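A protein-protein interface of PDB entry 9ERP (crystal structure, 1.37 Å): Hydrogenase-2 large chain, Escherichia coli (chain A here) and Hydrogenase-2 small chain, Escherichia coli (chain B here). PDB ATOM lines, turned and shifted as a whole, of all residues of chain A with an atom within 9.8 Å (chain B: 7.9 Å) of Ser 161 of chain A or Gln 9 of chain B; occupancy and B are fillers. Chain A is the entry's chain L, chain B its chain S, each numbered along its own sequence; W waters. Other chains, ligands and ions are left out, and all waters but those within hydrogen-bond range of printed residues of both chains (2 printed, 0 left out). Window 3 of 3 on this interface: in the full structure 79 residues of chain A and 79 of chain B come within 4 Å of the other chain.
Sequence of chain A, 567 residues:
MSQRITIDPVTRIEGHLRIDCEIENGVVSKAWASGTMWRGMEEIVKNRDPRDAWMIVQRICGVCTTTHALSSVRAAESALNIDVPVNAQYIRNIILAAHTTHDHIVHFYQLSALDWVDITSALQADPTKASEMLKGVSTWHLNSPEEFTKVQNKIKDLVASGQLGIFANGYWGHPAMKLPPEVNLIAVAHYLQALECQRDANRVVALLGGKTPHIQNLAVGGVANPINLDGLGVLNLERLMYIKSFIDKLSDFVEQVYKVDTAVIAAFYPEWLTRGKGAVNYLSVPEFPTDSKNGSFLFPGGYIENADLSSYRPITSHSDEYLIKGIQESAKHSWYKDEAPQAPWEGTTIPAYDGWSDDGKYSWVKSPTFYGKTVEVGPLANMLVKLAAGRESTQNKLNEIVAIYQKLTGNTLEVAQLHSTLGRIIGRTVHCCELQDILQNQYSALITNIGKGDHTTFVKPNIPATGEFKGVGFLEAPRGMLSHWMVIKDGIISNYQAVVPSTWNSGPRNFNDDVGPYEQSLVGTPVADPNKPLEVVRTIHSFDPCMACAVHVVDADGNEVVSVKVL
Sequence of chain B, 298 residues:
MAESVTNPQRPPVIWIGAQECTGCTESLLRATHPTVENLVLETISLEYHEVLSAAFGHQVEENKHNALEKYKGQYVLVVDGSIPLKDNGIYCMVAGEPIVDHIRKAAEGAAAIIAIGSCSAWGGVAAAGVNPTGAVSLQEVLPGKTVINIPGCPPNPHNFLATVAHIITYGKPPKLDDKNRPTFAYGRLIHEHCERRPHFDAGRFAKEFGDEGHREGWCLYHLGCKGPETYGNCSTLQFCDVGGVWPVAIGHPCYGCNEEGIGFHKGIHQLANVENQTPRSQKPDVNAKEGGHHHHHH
The side-chain hydroxyl of Ser 161 of chain A sits at hydrogen-bond distance from the guanidinium group of Arg 10 of chain B, at 3.1 Å. The backbone carbonyl oxygen of Ser 161 of chain A is in hydrogen-bond range of the side-chain amide nitrogen of Gln 9 of chain B (2.9 Å). The side-chain amide nitrogen of Gln 163 of chain A sits at hydrogen-bond distance from the side-chain hydroxyl of Tyr 71 of chain B, at 3.1 Å. OE1 of Gln 9 of chain B sits close to OE1 of Gln 163 of chain A. The backbone NH of Arg 10 of chain B sits at hydrogen-bond distance from the side-chain amide oxygen of Gln 163 of chain A (2.7 Å).
The guanidinium group (NH1) of Arg 10 of chain B lies within hydrogen-bond range of the backbone carbonyl oxygen (O) of Ile 44 of chain B. The side-chain hydroxyl (OG) of Ser 161 of chain A sits at hydrogen-bond distance from the backbone NH (N) of Gln 163 of chain A (3.0 Å). The side-chain hydroxyl (OH) of Tyr 71 of chain B sits at hydrogen-bond distance from the side-chain carboxylate (OE2) of Glu 47 of chain B, at 3.4 Å. O of Leu 158 of chain A sits at hydrogen-bond distance from OG of Ser 161 of chain A (2.7 Å). The backbone carbonyl oxygen (O) of Pro 11 of chain B sits at hydrogen-bond distance from the backbone NH (N) of Ser 45 of chain B (2.9 Å). NZ of Lys 70 of chain B is in hydrogen-bond range of OH of Tyr 71 of chain B (3.3 Å).
NH2 of Arg 10 of chain B touches CD1 of Leu 158 of chain A, at 3.9 Å. Leu 158 of chain A touches Leu 41 of chain B (CD1 to CD2, 3.9 Å). Gly 162 of chain A touches Lys 70 of chain B (O to NZ, 3.7 Å). CB of Gln 163 of chain A touches OG of Ser 45 of chain B, 3.5 Å away.
Water W1 lies within hydrogen-bond range of the backbone carbonyl oxygen of Gln 163 of chain A, the side-chain hydroxyl of Ser 45 of chain B, the guanidinium group of Arg 10 of chain B and the backbone NH of Gly 165 of chain A. Water W2 lies within hydrogen-bond range of the backbone carbonyl oxygen (O) of Pro 8 of chain B (2.7 Å), the guanidinium group (NE) of Arg 10 of chain B (2.8 Å), the side-chain amide oxygen (OE1) of Gln 163 of chain A (2.9 Å) and the side-chain hydroxyl (OG) of Ser 161 of chain A (3.4 Å).
Of the 13 printed residues of chain B, 6 touch a printed residue of chain A. Printed residues of chain B that touch a printed residue of chain A: Gln 9, Arg 10, Leu 41, Ser 45, Lys 70 and Tyr 71. Hydrophobic or aromatic side chains of chain B that line the printed part of chain A: Leu 41 and Tyr 71. Along chain B the printed residues that touch a printed residue of chain A span positions 9 to 71. Of the 15 printed residues of chain A, 4 touch a printed residue of chain B. Printed residues of chain A that touch a printed residue of chain B: Leu 158, Ser 161, Gly 162 and Gln 163. Hydrophobic or aromatic side chains of chain A that line the printed part of chain B: Leu 158.
Of chain B, only Gln 9 and Arg 10 come within 4 Å of Ser 161 of chain A. Gln 9 of chain B touches just these residues of chain A: Ser 161 and Gln 163. Of the printed residues of chain A, Ser 45 of chain B touches Gln 163 (3.5 Å). Of the printed residues of chain A, Lys 70 of chain B touches Gly 162. Printed residues of chain B within 4 Å of Gly 162 of chain A: Lys 70 (3.7 Å).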
ATOM      1  N   LEU A 123      -0.666  -1.661   1.055  1.00  0.00           N
ATOM      2  CA  LEU A 123       0.633  -2.077   1.584  1.00  0.00           C
ATOM      3  C   LEU A 123       1.345  -3.075   0.675  1.00  0.00           C
ATOM      4  O   LEU A 123       2.575  -3.203   0.768  1.00  0.00           O
ATOM      5  CB  LEU A 123       0.441  -2.684   2.972  1.00  0.00           C
ATOM      6  CG  LEU A 123       0.037  -1.687   4.056  1.00  0.00           C
ATOM      7  CD1 LEU A 123      -0.135  -2.434   5.373  1.00  0.00           C
ATOM      8  CD2 LEU A 123       1.076  -0.580   4.209  1.00  0.00           C
ATOM      9  N   ASN A 153       4.808   3.965   3.451  1.00  0.00           N
ATOM     10  CA  ASN A 153       5.496   3.785   4.728  1.00  0.00           C
ATOM     11  C   ASN A 153       4.714   4.391   5.887  1.00  0.00           C
ATOM     12  O   ASN A 153       4.767   3.858   6.999  1.00  0.00           O
ATOM     13  CB  ASN A 153       6.915   4.350   4.654  1.00  0.00           C
ATOM     14  CG  ASN A 153       7.829   3.499   3.797  1.00  0.00           C
ATOM     15  OD1 ASN A 153       7.568   2.321   3.579  1.00  0.00           O
ATOM     16  ND2 ASN A 153       8.888   4.102   3.288  1.00  0.00           N
ATOM     17  N   LYS A 154       3.986   5.496   5.657  1.00  0.00           N
ATOM     18  CA  LYS A 154       3.137   6.030   6.718  1.00  0.00           C
ATOM     19  C   LYS A 154       2.061   5.028   7.097  1.00  0.00           C
ATOM     20  O   LYS A 154       1.789   4.820   8.286  1.00  0.00           O
ATOM     21  CB  LYS A 154       2.490   7.360   6.312  1.00  0.00           C
ATOM     22  CG  LYS A 154       3.447   8.536   6.101  1.00  0.00           C
ATOM     23  CD  LYS A 154       2.667   9.773   5.591  1.00  0.00           C
ATOM     24  CE  LYS A 154       3.140  11.068   6.242  1.00  0.00           C
ATOM     25  NZ  LYS A 154       4.176  11.720   5.397  1.00  0.00           N
ATOM     26  N   ILE A 155       1.447   4.380   6.103  1.00  0.00           N
ATOM     27  CA  ILE A 155       0.441   3.373   6.400  1.00  0.00           C
ATOM     28  C   ILE A 155       1.085   2.199   7.126  1.00  0.00           C
ATOM     29  O   ILE A 155       0.542   1.680   8.102  1.00  0.00           O
ATOM     30  CB  ILE A 155      -0.261   2.881   5.122  1.00  0.00           C
ATOM     31  CG1 ILE A 155      -0.819   3.997   4.262  1.00  0.00           C
ATOM     32  CG2 ILE A 155      -1.372   1.878   5.502  1.00  0.00           C
ATOM     33  CD1 ILE A 155      -1.074   3.504   2.850  1.00  0.00           C
ATOM     34  N   LYS A 156       2.228   1.734   6.611  1.00  0.00           N
ATOM     35  CA  LYS A 156       2.964   0.643   7.246  1.00  0.00           C
ATOM     36  C   LYS A 156       3.183   0.933   8.726  1.00  0.00           C
ATOM     37  O   LYS A 156       2.908   0.087   9.581  1.00  0.00           O
ATOM     38  CB  LYS A 156       4.321   0.453   6.543  1.00  0.00           C
ATOM     39  CG  LYS A 156       5.015  -0.892   6.812  1.00  0.00           C
ATOM     40  CD  LYS A 156       6.201  -1.181   5.853  1.00  0.00           C
ATOM     41  CE  LYS A 156       5.884  -0.842   4.394  1.00  0.00           C
ATOM     42  NZ  LYS A 156       6.544  -1.718   3.349  1.00  0.00           N
ATOM     43  N   ASP A 157       3.686   2.121   9.042  1.00  0.00           N
ATOM     44  CA  ASP A 157       3.989   2.460  10.434  1.00  0.00           C
ATOM     45  C   ASP A 157       2.725   2.492  11.279  1.00  0.00           C
ATOM     46  O   ASP A 157       2.719   2.025  12.426  1.00  0.00           O
ATOM     47  CB  ASP A 157       4.700   3.820  10.525  1.00  0.00           C
ATOM     48  CG  ASP A 157       6.119   3.782   9.980  1.00  0.00           C
ATOM     49  OD1 ASP A 157       6.658   2.679   9.788  1.00  0.00           O
ATOM     50  OD2 ASP A 157       6.673   4.861   9.730  1.00  0.00           O
ATOM     51  N   LEU A 158       1.647   3.062  10.737  1.00  0.00           N
ATOM     52  CA  LEU A 158       0.386   3.089  11.458  1.00  0.00           C
ATOM     53  C   LEU A 158      -0.067   1.675  11.796  1.00  0.00           C
ATOM     54  O   LEU A 158      -0.440   1.386  12.939  1.00  0.00           O
ATOM     55  CB  LEU A 158      -0.675   3.808  10.607  1.00  0.00           C
ATOM     56  CG  LEU A 158      -2.093   3.791  11.194  1.00  0.00           C
ATOM     57  CD1 LEU A 158      -2.392   5.094  11.894  1.00  0.00           C
ATOM     58  CD2 LEU A 158      -3.100   3.514  10.102  1.00  0.00           C
ATOM     59  N   VAL A 159      -0.075   0.783  10.805  1.00  0.00           N
ATOM     60  CA  VAL A 159      -0.528  -0.592  11.044  1.00  0.00           C
ATOM     61  C   VAL A 159       0.377  -1.274  12.062  1.00  0.00           C
ATOM     62  O   VAL A 159      -0.099  -1.946  12.989  1.00  0.00           O
ATOM     63  CB  VAL A 159      -0.597  -1.364   9.714  1.00  0.00           C
ATOM     64  CG1 VAL A 159      -0.889  -2.859   9.935  1.00  0.00           C
ATOM     65  CG2 VAL A 159      -1.655  -0.754   8.792  1.00  0.00           C
ATOM     66  N   ALA A 160       1.685  -1.080  11.930  1.00  0.00           N
ATOM     67  CA  ALA A 160       2.633  -1.730  12.828  1.00  0.00           C
ATOM     68  C   ALA A 160       2.459  -1.270  14.265  1.00  0.00           C
ATOM     69  O   ALA A 160       2.759  -2.031  15.190  1.00  0.00           O
ATOM     70  CB  ALA A 160       4.062  -1.442  12.369  1.00  0.00           C
ATOM     71  N   SER A 161       1.978  -0.041  14.479  1.00  0.00           N
ATOM     72  CA  SER A 161       1.795   0.455  15.831  1.00  0.00           C
ATOM     73  C   SER A 161       0.669  -0.259  16.569  1.00  0.00           C
ATOM     74  O   SER A 161       0.563  -0.123  17.795  1.00  0.00           O
ATOM     75  CB  SER A 161       1.471   1.949  15.812  1.00  0.00           C
ATOM     76  OG  SER A 161       0.116   2.169  15.443  1.00  0.00           O
ATOM     77  N   GLY A 162      -0.188  -0.988  15.866  1.00  0.00           N
ATOM     78  CA  GLY A 162      -1.355  -1.570  16.490  1.00  0.00           C
ATOM     79  C   GLY A 162      -2.435  -0.579  16.870  1.00  0.00           C
ATOM     80  O   GLY A 162      -3.422  -0.978  17.491  1.00  0.00           O
ATOM     81  N   GLN A 163      -2.262   0.704  16.540  1.00  0.00           N
ATOM     82  CA  GLN A 163      -3.269   1.740  16.800  1.00  0.00           C
ATOM     83  C   GLN A 163      -3.762   2.278  15.459  1.00  0.00           C
ATOM     84  O   GLN A 163      -3.243   3.276  14.950  1.00  0.00           O
ATOM     85  CB  GLN A 163      -2.697   2.872  17.636  1.00  0.00           C
ATOM     86  CG  GLN A 163      -2.147   2.457  18.977  1.00  0.00           C
ATOM     87  CD  GLN A 163      -1.617   3.657  19.738  1.00  0.00           C
ATOM     88  OE1 GLN A 163      -0.603   4.243  19.359  1.00  0.00           O
ATOM     89  NE2 GLN A 163      -2.350   4.071  20.760  1.00  0.00           N
ATOM     90  N   LEU A 164      -4.771   1.610  14.892  1.00  0.00           N
ATOM     91  CA  LEU A 164      -5.262   1.971  13.568  1.00  0.00           C
ATOM     92  C   LEU A 164      -6.196   3.180  13.596  1.00  0.00           C
ATOM     93  O   LEU A 164      -6.395   3.815  12.553  1.00  0.00           O
ATOM     94  CB  LEU A 164      -5.994   0.789  12.937  1.00  0.00           C
ATOM     95  CG  LEU A 164      -5.152  -0.292  12.264  1.00  0.00           C
ATOM     96  CD1 LEU A 164      -4.349   0.254  11.123  1.00  0.00           C
ATOM     97  CD2 LEU A 164      -4.238  -0.936  13.272  1.00  0.00           C
ATOM     98  N   GLY A 165      -6.761   3.508  14.748  1.00  0.00           N
ATOM     99  CA  GLY A 165      -7.546   4.733  14.861  1.00  0.00           C
ATOM    100  C   GLY A 165      -8.692   4.772  13.866  1.00  0.00           C
ATOM    101  O   GLY A 165      -9.524   3.863  13.816  1.00  0.00           O
ATOM    102  N   PHE A 167      -8.806   4.107  10.916  1.00  0.00           N
ATOM    103  CA  PHE A 167      -8.762   2.981   9.995  1.00  0.00           C
ATOM    104  C   PHE A 167      -9.088   1.647  10.653  1.00  0.00           C
ATOM    105  O   PHE A 167      -9.159   0.630   9.961  1.00  0.00           O
ATOM    106  CB  PHE A 167      -7.369   2.926   9.378  1.00  0.00           C
ATOM    107  CG  PHE A 167      -7.010   4.172   8.665  1.00  0.00           C
ATOM    108  CD1 PHE A 167      -7.545   4.440   7.415  1.00  0.00           C
ATOM    109  CD2 PHE A 167      -6.214   5.130   9.270  1.00  0.00           C
ATOM    110  CE1 PHE A 167      -7.246   5.616   6.756  1.00  0.00           C
ATOM    111  CE2 PHE A 167      -5.908   6.309   8.616  1.00  0.00           C
ATOM    112  CZ  PHE A 167      -6.428   6.555   7.357  1.00  0.00           C
ATOM    113  N   PRO B   8       6.410   4.570  18.276  1.00  0.00           N
ATOM    114  CA  PRO B   8       5.870   4.670  19.637  1.00  0.00           C
ATOM    115  C   PRO B   8       4.350   4.766  19.682  1.00  0.00           C
ATOM    116  O   PRO B   8       3.718   5.204  18.715  1.00  0.00           O
ATOM    117  CB  PRO B   8       6.491   5.971  20.151  1.00  0.00           C
ATOM    118  CG  PRO B   8       6.570   6.836  18.922  1.00  0.00           C
ATOM    119  CD  PRO B   8       6.851   5.883  17.763  1.00  0.00           C
ATOM    120  N   GLN B   9       3.771   4.357  20.803  1.00  0.00           N
ATOM    121  CA  GLN B   9       2.335   4.461  20.983  1.00  0.00           C
ATOM    122  C   GLN B   9       1.930   5.924  21.105  1.00  0.00           C
ATOM    123  O   GLN B   9       2.690   6.760  21.590  1.00  0.00           O
ATOM    124  CB  GLN B   9       1.907   3.715  22.235  1.00  0.00           C
ATOM    125  CG  GLN B   9       2.179   2.234  22.144  1.00  0.00           C
ATOM    126  CD  GLN B   9       1.314   1.569  21.099  1.00  0.00           C
ATOM    127  OE1 GLN B   9       0.106   1.446  21.268  1.00  0.00           O
ATOM    128  NE2 GLN B   9       1.928   1.155  19.998  1.00  0.00           N
ATOM    129  N   ARG B  10       0.713   6.228  20.653  1.00  0.00           N
ATOM    130  CA  ARG B  10       0.194   7.584  20.700  1.00  0.00           C
ATOM    131  C   ARG B  10      -0.971   7.680  21.677  1.00  0.00           C
ATOM    132  O   ARG B  10      -1.727   6.717  21.851  1.00  0.00           O
ATOM    133  CB  ARG B  10      -0.266   8.046  19.307  1.00  0.00           C
ATOM    134  CG  ARG B  10       0.873   8.297  18.333  1.00  0.00           C
ATOM    135  CD  ARG B  10       0.415   8.280  16.871  1.00  0.00           C
ATOM    136  NE  ARG B  10       0.251   6.922  16.382  1.00  0.00           N
ATOM    137  CZ  ARG B  10      -0.858   6.422  15.854  1.00  0.00           C
ATOM    138  NH1 ARG B  10      -1.945   7.166  15.670  1.00  0.00           N
ATOM    139  NH2 ARG B  10      -0.874   5.152  15.467  1.00  0.00           N
ATOM    140  N   PRO B  11      -1.165   8.839  22.302  1.00  0.00           N
ATOM    141  CA  PRO B  11      -2.247   8.985  23.296  1.00  0.00           C
ATOM    142  C   PRO B  11      -3.609   8.859  22.648  1.00  0.00           C
ATOM    143  O   PRO B  11      -3.857   9.480  21.600  1.00  0.00           O
ATOM    144  CB  PRO B  11      -2.034  10.394  23.874  1.00  0.00           C
ATOM    145  CG  PRO B  11      -0.907  10.984  23.189  1.00  0.00           C
ATOM    146  CD  PRO B  11      -0.271  10.016  22.242  1.00  0.00           C
ATOM    147  N   PRO B  12      -4.514   8.095  23.256  1.00  0.00           N
ATOM    148  CA  PRO B  12      -5.824   7.837  22.640  1.00  0.00           C
ATOM    149  C   PRO B  12      -6.846   8.930  22.922  1.00  0.00           C
ATOM    150  O   PRO B  12      -6.890   9.514  24.012  1.00  0.00           O
ATOM    151  CB  PRO B  12      -6.269   6.527  23.307  1.00  0.00           C
ATOM    152  CG  PRO B  12      -5.632   6.606  24.688  1.00  0.00           C
ATOM    153  CD  PRO B  12      -4.314   7.292  24.483  1.00  0.00           C
ATOM    154  N   LEU B  41      -2.124  10.850  12.577  1.00  0.00           N
ATOM    155  CA  LEU B  41      -1.054   9.888  12.320  1.00  0.00           C
ATOM    156  C   LEU B  41       0.103   9.985  13.300  1.00  0.00           C
ATOM    157  O   LEU B  41       0.805   8.982  13.493  1.00  0.00           O
ATOM    158  CB  LEU B  41      -0.496  10.044  10.899  1.00  0.00           C
ATOM    159  CG  LEU B  41      -1.485   9.785   9.758  1.00  0.00           C
ATOM    160  CD1 LEU B  41      -0.824  10.045   8.408  1.00  0.00           C
ATOM    161  CD2 LEU B  41      -2.077   8.373   9.805  1.00  0.00           C
ATOM    162  N   GLU B  42       0.348  11.157  13.905  1.00  0.00           N
ATOM    163  CA  GLU B  42       1.541  11.354  14.742  1.00  0.00           C
ATOM    164  C   GLU B  42       1.241  11.790  16.171  1.00  0.00           C
ATOM    165  O   GLU B  42       1.883  11.311  17.103  1.00  0.00           O
ATOM    166  CB  GLU B  42       2.506  12.392  14.117  1.00  0.00           C
ATOM    167  CG  GLU B  42       2.631  12.351  12.598  1.00  0.00           C
ATOM    168  CD  GLU B  42       3.487  11.211  12.100  1.00  0.00           C
ATOM    169  OE1 GLU B  42       4.150  10.557  12.935  1.00  0.00           O
ATOM    170  OE2 GLU B  42       3.495  10.960  10.865  1.00  0.00           O
ATOM    171  N   THR B  43       0.293  12.701  16.374  1.00  0.00           N
ATOM    172  CA  THR B  43       0.095  13.290  17.699  1.00  0.00           C
ATOM    173  C   THR B  43      -0.725  12.396  18.615  1.00  0.00           C
ATOM    174  O   THR B  43      -0.381  12.199  19.790  1.00  0.00           O
ATOM    175  CB  THR B  43      -0.596  14.656  17.577  1.00  0.00           C
ATOM    176  OG1 THR B  43       0.053  15.431  16.562  1.00  0.00           O
ATOM    177  CG2 THR B  43      -0.577  15.396  18.924  1.00  0.00           C
ATOM    178  N   ILE B  44      -1.851  11.902  18.119  1.00  0.00           N
ATOM    179  CA  ILE B  44      -2.797  11.117  18.886  1.00  0.00           C
ATOM    180  C   ILE B  44      -3.146   9.864  18.096  1.00  0.00           C
ATOM    181  O   ILE B  44      -2.818   9.727  16.914  1.00  0.00           O
ATOM    182  CB  ILE B  44      -4.080  11.913  19.234  1.00  0.00           C
ATOM    183  CG1 ILE B  44      -4.856  12.241  17.936  1.00  0.00           C
ATOM    184  CG2 ILE B  44      -3.762  13.172  20.033  1.00  0.00           C
ATOM    185  CD1 ILE B  44      -6.273  12.709  18.163  1.00  0.00           C
ATOM    186  N   SER B  45      -3.837   8.963  18.772  1.00  0.00           N
ATOM    187  CA  SER B  45      -4.590   7.903  18.127  1.00  0.00           C
ATOM    188  C   SER B  45      -6.065   8.253  18.299  1.00  0.00           C
ATOM    189  O   SER B  45      -6.596   8.226  19.417  1.00  0.00           O
ATOM    190  CB  SER B  45      -4.298   6.533  18.736  1.00  0.00           C
ATOM    191  OG  SER B  45      -4.904   5.543  17.921  1.00  0.00           O
ATOM    192  N   GLU B  47      -9.323   7.161  18.308  1.00  0.00           N
ATOM    193  CA  GLU B  47      -9.877   5.818  18.408  1.00  0.00           C
ATOM    194  C   GLU B  47     -11.355   5.775  18.077  1.00  0.00           C
ATOM    195  O   GLU B  47     -11.888   4.702  17.766  1.00  0.00           O
ATOM    196  CB  GLU B  47      -9.693   5.302  19.838  1.00  0.00           C
ATOM    197  CG  GLU B  47      -8.259   5.127  20.221  1.00  0.00           C
ATOM    198  CD  GLU B  47      -7.635   3.900  19.608  1.00  0.00           C
ATOM    199  OE1 GLU B  47      -8.363   2.903  19.418  1.00  0.00           O
ATOM    200  OE2 GLU B  47      -6.432   3.942  19.315  1.00  0.00           O
ATOM    201  N   LYS B  70      -9.454  -1.042  26.392  1.00  0.00           N
ATOM    202  CA  LYS B  70      -8.005  -1.037  26.234  1.00  0.00           C
ATOM    203  C   LYS B  70      -7.372   0.194  26.870  1.00  0.00           C
ATOM    204  O   LYS B  70      -6.271   0.115  27.432  1.00  0.00           O
ATOM    205  CB  LYS B  70      -7.647  -1.118  24.747  1.00  0.00           C
ATOM    206  CG  LYS B  70      -6.153  -1.079  24.425  1.00  0.00           C
ATOM    207  CD  LYS B  70      -5.920  -1.250  22.926  1.00  0.00           C
ATOM    208  CE  LYS B  70      -4.459  -1.384  22.587  1.00  0.00           C
ATOM    209  NZ  LYS B  70      -4.186  -1.226  21.123  1.00  0.00           N
ATOM    210  N   TYR B  71      -8.050   1.344  26.796  1.00  0.00           N
ATOM    211  CA  TYR B  71      -7.461   2.614  27.195  1.00  0.00           C
ATOM    212  C   TYR B  71      -8.129   3.216  28.425  1.00  0.00           C
ATOM    213  O   TYR B  71      -7.997   4.421  28.673  1.00  0.00           O
ATOM    214  CB  TYR B  71      -7.514   3.586  26.014  1.00  0.00           C
ATOM    215  CG  TYR B  71      -6.727   3.159  24.796  1.00  0.00           C
ATOM    216  CD1 TYR B  71      -5.333   3.043  24.831  1.00  0.00           C
ATOM    217  CD2 TYR B  71      -7.374   2.863  23.604  1.00  0.00           C
ATOM    218  CE1 TYR B  71      -4.630   2.656  23.710  1.00  0.00           C
ATOM    219  CE2 TYR B  71      -6.675   2.487  22.484  1.00  0.00           C
ATOM    220  CZ  TYR B  71      -5.308   2.382  22.534  1.00  0.00           C
ATOM    221  OH  TYR B  71      -4.623   2.004  21.400  1.00  0.00           O
HETATM  222  O   HOH W   1      -4.348   5.686  15.141  1.00  0.00           O
HETATM  223  O   HOH W   2       1.468   4.581  17.379  1.00  0.00           O
